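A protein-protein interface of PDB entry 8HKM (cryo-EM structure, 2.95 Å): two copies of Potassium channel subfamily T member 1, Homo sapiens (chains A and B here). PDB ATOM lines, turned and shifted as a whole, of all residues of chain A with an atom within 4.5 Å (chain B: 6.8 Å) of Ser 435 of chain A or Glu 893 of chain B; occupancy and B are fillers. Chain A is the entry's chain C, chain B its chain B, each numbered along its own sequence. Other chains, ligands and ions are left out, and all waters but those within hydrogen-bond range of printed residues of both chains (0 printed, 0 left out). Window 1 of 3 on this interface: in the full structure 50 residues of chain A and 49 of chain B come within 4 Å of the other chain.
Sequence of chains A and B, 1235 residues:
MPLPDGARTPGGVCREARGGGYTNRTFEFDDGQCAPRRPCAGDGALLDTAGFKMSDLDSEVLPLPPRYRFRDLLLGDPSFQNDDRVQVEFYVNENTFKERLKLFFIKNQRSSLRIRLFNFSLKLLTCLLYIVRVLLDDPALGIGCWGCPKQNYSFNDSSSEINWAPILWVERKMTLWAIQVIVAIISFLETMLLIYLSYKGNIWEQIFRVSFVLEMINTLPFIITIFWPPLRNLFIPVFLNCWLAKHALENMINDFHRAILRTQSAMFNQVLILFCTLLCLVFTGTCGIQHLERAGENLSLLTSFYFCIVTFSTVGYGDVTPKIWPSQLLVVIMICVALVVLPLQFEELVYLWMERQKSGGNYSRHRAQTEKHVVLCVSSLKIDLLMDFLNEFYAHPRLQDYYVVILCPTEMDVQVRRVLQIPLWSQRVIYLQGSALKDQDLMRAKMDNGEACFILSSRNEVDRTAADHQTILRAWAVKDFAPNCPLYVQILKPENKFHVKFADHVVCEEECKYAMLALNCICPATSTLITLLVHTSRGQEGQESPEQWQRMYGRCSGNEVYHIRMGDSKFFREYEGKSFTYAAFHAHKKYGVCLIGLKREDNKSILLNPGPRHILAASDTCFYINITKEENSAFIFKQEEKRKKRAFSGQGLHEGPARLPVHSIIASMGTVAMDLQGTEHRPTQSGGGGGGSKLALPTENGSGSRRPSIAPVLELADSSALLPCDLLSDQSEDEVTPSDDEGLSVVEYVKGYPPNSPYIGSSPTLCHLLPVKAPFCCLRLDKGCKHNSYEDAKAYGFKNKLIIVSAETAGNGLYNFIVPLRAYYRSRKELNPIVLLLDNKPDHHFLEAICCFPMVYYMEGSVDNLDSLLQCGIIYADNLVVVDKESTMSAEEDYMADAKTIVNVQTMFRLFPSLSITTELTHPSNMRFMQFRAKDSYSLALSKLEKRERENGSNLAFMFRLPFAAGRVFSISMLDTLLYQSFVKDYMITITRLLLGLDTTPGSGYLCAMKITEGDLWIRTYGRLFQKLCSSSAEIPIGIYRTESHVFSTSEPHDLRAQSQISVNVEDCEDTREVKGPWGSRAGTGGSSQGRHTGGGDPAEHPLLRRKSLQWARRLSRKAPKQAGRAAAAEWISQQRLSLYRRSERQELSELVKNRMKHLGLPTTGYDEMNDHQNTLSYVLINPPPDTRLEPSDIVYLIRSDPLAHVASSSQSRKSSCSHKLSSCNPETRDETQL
Among the printed residues, pairs that only touch across the chains: Pro 409 of chain A with Glu 893 of chain B, Leu 437 of chain A with Tyr 895 of chain B, Leu 437 of chain A with Met 896 of chain B, Lys 438 of chain A with Tyr 895 of chain B and Arg 474 of chain A with Met 896 of chain B.
Hydrophobic or aromatic side chains of chain B within 4 Å of the printed part of chain A: Tyr 895 and Met 896.
Hydrophobic or aromatic side chains of chain A within 4 Å of the printed part of chain B: Pro 409 and Leu 437.
Among the printed residues, 8 pairs touch across the chains.
Of the printed residues of chain B, Lys 438 of chain A touches Tyr 895.
Printed residues of chain B within 4 Å of Leu 437 of chain A: Tyr 895 and Met 896.
Printed residues of chain A within 4 Å of Glu 892 of chain B: Pro 409.
Of the printed residues of chain B, Arg 474 of chain A touches Glu 893 and Met 896.
Leu 407 of chain A touches none of the printed residues of chain B.
The nearest residue of chain A that does not touch Glu 893 of chain B is Ala 436 of chain A (4.3 Å).
The nearest printed residue of chain A that does not touch Glu 892 of chain B is Ser 435 of chain A (5.9 Å).
No position is printed for both chains.
The backbone NH of Ser 435 of chain A is in hydrogen-bond range of the side-chain carboxylate of Asp 441 of chain A, at 2.8 Å.
The side-chain carboxylate (OD2) of Asp 441 of chain A lies within salt-bridge range of the side-chain amino group (NZ) of Lys 438 of chain A.
The side-chain hydroxyl (OG) of Ser 435 of chain A lies within hydrogen-bond range of the side-chain carboxylate (OE2) of Glu 893 of chain B, at 3.1 Å.
OE1 of Glu 893 of chain B is in salt-bridge range of NH2 of Arg 474 of chain A (2.7 Å).
The backbone carbonyl oxygen (O) of Pro 409 of chain A sits close to the side-chain carboxylate (OE1) of Glu 892 of chain B, at 3.0 Å.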
ATOM      1  N   LEU A 407     -10.242 -32.798 -25.287  1.00  0.00           N
ATOM      2  CA  LEU A 407      -9.580 -31.515 -25.076  1.00  0.00           C
ATOM      3  C   LEU A 407      -8.112 -31.676 -25.460  1.00  0.00           C
ATOM      4  O   LEU A 407      -7.262 -31.966 -24.614  1.00  0.00           O
ATOM      5  CB  LEU A 407      -9.742 -31.054 -23.631  1.00  0.00           C
ATOM      6  CG  LEU A 407      -9.531 -29.567 -23.349  1.00  0.00           C
ATOM      7  CD1 LEU A 407     -10.748 -28.769 -23.781  1.00  0.00           C
ATOM      8  CD2 LEU A 407      -9.235 -29.344 -21.877  1.00  0.00           C
ATOM      9  N   PRO A 409      -4.849 -29.729 -27.458  1.00  0.00           N
ATOM     10  CA  PRO A 409      -4.449 -28.384 -27.898  1.00  0.00           C
ATOM     11  C   PRO A 409      -4.102 -28.291 -29.374  1.00  0.00           C
ATOM     12  O   PRO A 409      -3.822 -27.184 -29.851  1.00  0.00           O
ATOM     13  CB  PRO A 409      -3.223 -28.086 -27.028  1.00  0.00           C
ATOM     14  CG  PRO A 409      -2.641 -29.428 -26.756  1.00  0.00           C
ATOM     15  CD  PRO A 409      -3.807 -30.377 -26.643  1.00  0.00           C
ATOM     16  N   GLY A 434      -8.062 -26.982 -27.070  1.00  0.00           N
ATOM     17  CA  GLY A 434      -7.732 -26.132 -25.943  1.00  0.00           C
ATOM     18  C   GLY A 434      -6.793 -26.849 -25.001  1.00  0.00           C
ATOM     19  O   GLY A 434      -6.388 -27.993 -25.233  1.00  0.00           O
ATOM     20  N   SER A 435      -6.451 -26.153 -23.922  1.00  0.00           N
ATOM     21  CA  SER A 435      -5.518 -26.649 -22.924  1.00  0.00           C
ATOM     22  C   SER A 435      -6.224 -26.828 -21.587  1.00  0.00           C
ATOM     23  O   SER A 435      -7.074 -26.016 -21.208  1.00  0.00           O
ATOM     24  CB  SER A 435      -4.334 -25.692 -22.760  1.00  0.00           C
ATOM     25  OG  SER A 435      -3.558 -25.637 -23.943  1.00  0.00           O
ATOM     26  N   ALA A 436      -5.868 -27.900 -20.877  1.00  0.00           N
ATOM     27  CA  ALA A 436      -6.388 -28.109 -19.532  1.00  0.00           C
ATOM     28  C   ALA A 436      -5.901 -27.050 -18.554  1.00  0.00           C
ATOM     29  O   ALA A 436      -6.518 -26.867 -17.501  1.00  0.00           O
ATOM     30  CB  ALA A 436      -6.000 -29.498 -19.023  1.00  0.00           C
ATOM     31  N   LEU A 437      -4.814 -26.349 -18.877  1.00  0.00           N
ATOM     32  CA  LEU A 437      -4.297 -25.298 -18.012  1.00  0.00           C
ATOM     33  C   LEU A 437      -5.030 -23.974 -18.182  1.00  0.00           C
ATOM     34  O   LEU A 437      -4.810 -23.057 -17.382  1.00  0.00           O
ATOM     35  CB  LEU A 437      -2.802 -25.094 -18.268  1.00  0.00           C
ATOM     36  CG  LEU A 437      -1.846 -25.785 -17.292  1.00  0.00           C
ATOM     37  CD1 LEU A 437      -2.099 -27.283 -17.243  1.00  0.00           C
ATOM     38  CD2 LEU A 437      -0.400 -25.496 -17.660  1.00  0.00           C
ATOM     39  N   LYS A 438      -5.887 -23.850 -19.191  1.00  0.00           N
ATOM     40  CA  LYS A 438      -6.693 -22.654 -19.404  1.00  0.00           C
ATOM     41  C   LYS A 438      -8.106 -22.929 -18.906  1.00  0.00           C
ATOM     42  O   LYS A 438      -8.748 -23.887 -19.349  1.00  0.00           O
ATOM     43  CB  LYS A 438      -6.703 -22.248 -20.878  1.00  0.00           C
ATOM     44  CG  LYS A 438      -5.322 -22.104 -21.497  1.00  0.00           C
ATOM     45  CD  LYS A 438      -5.271 -20.936 -22.473  1.00  0.00           C
ATOM     46  CE  LYS A 438      -6.068 -21.214 -23.736  1.00  0.00           C
ATOM     47  NZ  LYS A 438      -5.616 -22.454 -24.425  1.00  0.00           N
ATOM     48  N   ASP A 441     -11.084 -23.149 -21.509  1.00  0.00           N
ATOM     49  CA  ASP A 441     -11.193 -24.452 -22.159  1.00  0.00           C
ATOM     50  C   ASP A 441     -11.785 -25.482 -21.207  1.00  0.00           C
ATOM     51  O   ASP A 441     -12.582 -26.334 -21.617  1.00  0.00           O
ATOM     52  CB  ASP A 441      -9.825 -24.911 -22.662  1.00  0.00           C
ATOM     53  CG  ASP A 441      -9.145 -23.873 -23.530  1.00  0.00           C
ATOM     54  OD1 ASP A 441      -9.853 -23.117 -24.227  1.00  0.00           O
ATOM     55  OD2 ASP A 441      -7.898 -23.822 -23.522  1.00  0.00           O
ATOM     56  N   ARG A 474      -1.552 -31.094 -16.076  1.00  0.00           N
ATOM     57  CA  ARG A 474      -2.940 -31.278 -16.484  1.00  0.00           C
ATOM     58  C   ARG A 474      -3.772 -31.906 -15.375  1.00  0.00           C
ATOM     59  O   ARG A 474      -4.926 -31.514 -15.170  1.00  0.00           O
ATOM     60  CB  ARG A 474      -3.010 -32.129 -17.751  1.00  0.00           C
ATOM     61  CG  ARG A 474      -2.717 -31.358 -19.024  1.00  0.00           C
ATOM     62  CD  ARG A 474      -2.497 -32.288 -20.202  1.00  0.00           C
ATOM     63  NE  ARG A 474      -2.007 -31.572 -21.373  1.00  0.00           N
ATOM     64  CZ  ARG A 474      -1.279 -32.118 -22.337  1.00  0.00           C
ATOM     65  NH1 ARG A 474      -0.932 -33.395 -22.300  1.00  0.00           N
ATOM     66  NH2 ARG A 474      -0.892 -31.368 -23.363  1.00  0.00           N
ATOM     67  N   ALA B 891       7.514 -24.761 -27.342  1.00  0.00           N
ATOM     68  CA  ALA B 891       6.290 -25.507 -27.072  1.00  0.00           C
ATOM     69  C   ALA B 891       5.081 -24.811 -27.686  1.00  0.00           C
ATOM     70  O   ALA B 891       4.945 -23.591 -27.592  1.00  0.00           O
ATOM     71  CB  ALA B 891       6.096 -25.683 -25.574  1.00  0.00           C
ATOM     72  N   GLU B 892       4.200 -25.590 -28.316  1.00  0.00           N
ATOM     73  CA  GLU B 892       2.999 -25.008 -28.907  1.00  0.00           C
ATOM     74  C   GLU B 892       1.986 -24.651 -27.826  1.00  0.00           C
ATOM     75  O   GLU B 892       1.495 -23.518 -27.769  1.00  0.00           O
ATOM     76  CB  GLU B 892       2.404 -25.968 -29.945  1.00  0.00           C
ATOM     77  CG  GLU B 892       0.955 -25.686 -30.360  1.00  0.00           C
ATOM     78  CD  GLU B 892      -0.076 -26.265 -29.407  1.00  0.00           C
ATOM     79  OE1 GLU B 892      -1.202 -25.729 -29.350  1.00  0.00           O
ATOM     80  OE2 GLU B 892       0.243 -27.255 -28.718  1.00  0.00           O
ATOM     81  N   GLU B 893       1.658 -25.609 -26.956  1.00  0.00           N
ATOM     82  CA  GLU B 893       0.780 -25.313 -25.830  1.00  0.00           C
ATOM     83  C   GLU B 893       1.526 -24.382 -24.882  1.00  0.00           C
ATOM     84  O   GLU B 893       2.478 -24.793 -24.211  1.00  0.00           O
ATOM     85  CB  GLU B 893       0.327 -26.597 -25.128  1.00  0.00           C
ATOM     86  CG  GLU B 893      -0.368 -26.366 -23.793  1.00  0.00           C
ATOM     87  CD  GLU B 893      -0.981 -27.632 -23.220  1.00  0.00           C
ATOM     88  OE1 GLU B 893      -0.697 -28.728 -23.747  1.00  0.00           O
ATOM     89  OE2 GLU B 893      -1.756 -27.529 -22.245  1.00  0.00           O
ATOM     90  N   ASP B 894       1.098 -23.120 -24.840  1.00  0.00           N
ATOM     91  CA  ASP B 894       1.941 -22.053 -24.304  1.00  0.00           C
ATOM     92  C   ASP B 894       2.140 -22.178 -22.800  1.00  0.00           C
ATOM     93  O   ASP B 894       3.237 -21.920 -22.292  1.00  0.00           O
ATOM     94  CB  ASP B 894       1.336 -20.698 -24.662  1.00  0.00           C
ATOM     95  CG  ASP B 894       1.506 -20.363 -26.126  1.00  0.00           C
ATOM     96  OD1 ASP B 894       2.612 -20.586 -26.658  1.00  0.00           O
ATOM     97  OD2 ASP B 894       0.534 -19.887 -26.749  1.00  0.00           O
ATOM     98  N   TYR B 895       1.093 -22.556 -22.068  1.00  0.00           N
ATOM     99  CA  TYR B 895       1.190 -22.592 -20.615  1.00  0.00           C
ATOM    100  C   TYR B 895       2.062 -23.737 -20.114  1.00  0.00           C
ATOM    101  O   TYR B 895       2.385 -23.771 -18.922  1.00  0.00           O
ATOM    102  CB  TYR B 895      -0.208 -22.678 -20.004  1.00  0.00           C
ATOM    103  CG  TYR B 895      -0.845 -21.320 -19.796  1.00  0.00           C
ATOM    104  CD1 TYR B 895      -0.571 -20.562 -18.667  1.00  0.00           C
ATOM    105  CD2 TYR B 895      -1.720 -20.797 -20.738  1.00  0.00           C
ATOM    106  CE1 TYR B 895      -1.150 -19.318 -18.484  1.00  0.00           C
ATOM    107  CE2 TYR B 895      -2.305 -19.556 -20.560  1.00  0.00           C
ATOM    108  CZ  TYR B 895      -2.016 -18.821 -19.430  1.00  0.00           C
ATOM    109  OH  TYR B 895      -2.591 -17.585 -19.242  1.00  0.00           O
ATOM    110  N   MET B 896       2.443 -24.669 -20.988  1.00  0.00           N
ATOM    111  CA  MET B 896       3.352 -25.756 -20.642  1.00  0.00           C
ATOM    112  C   MET B 896       4.805 -25.311 -20.549  1.00  0.00           C
ATOM    113  O   MET B 896       5.677 -26.160 -20.338  1.00  0.00           O
ATOM    114  CB  MET B 896       3.242 -26.889 -21.666  1.00  0.00           C
ATOM    115  CG  MET B 896       2.006 -27.758 -21.537  1.00  0.00           C
ATOM    116  SD  MET B 896       1.879 -28.578 -19.942  1.00  0.00           S
ATOM    117  CE  MET B 896       0.102 -28.684 -19.775  1.00  0.00           C
ATOM    118  N   ALA B 897       5.091 -24.018 -20.715  1.00  0.00           N
ATOM    119  CA  ALA B 897       6.475 -23.558 -20.694  1.00  0.00           C
ATOM    120  C   ALA B 897       7.115 -23.784 -19.329  1.00  0.00           C
ATOM    121  O   ALA B 897       8.302 -24.120 -19.239  1.00  0.00           O
ATOM    122  CB  ALA B 897       6.544 -22.081 -21.083  1.00  0.00           C
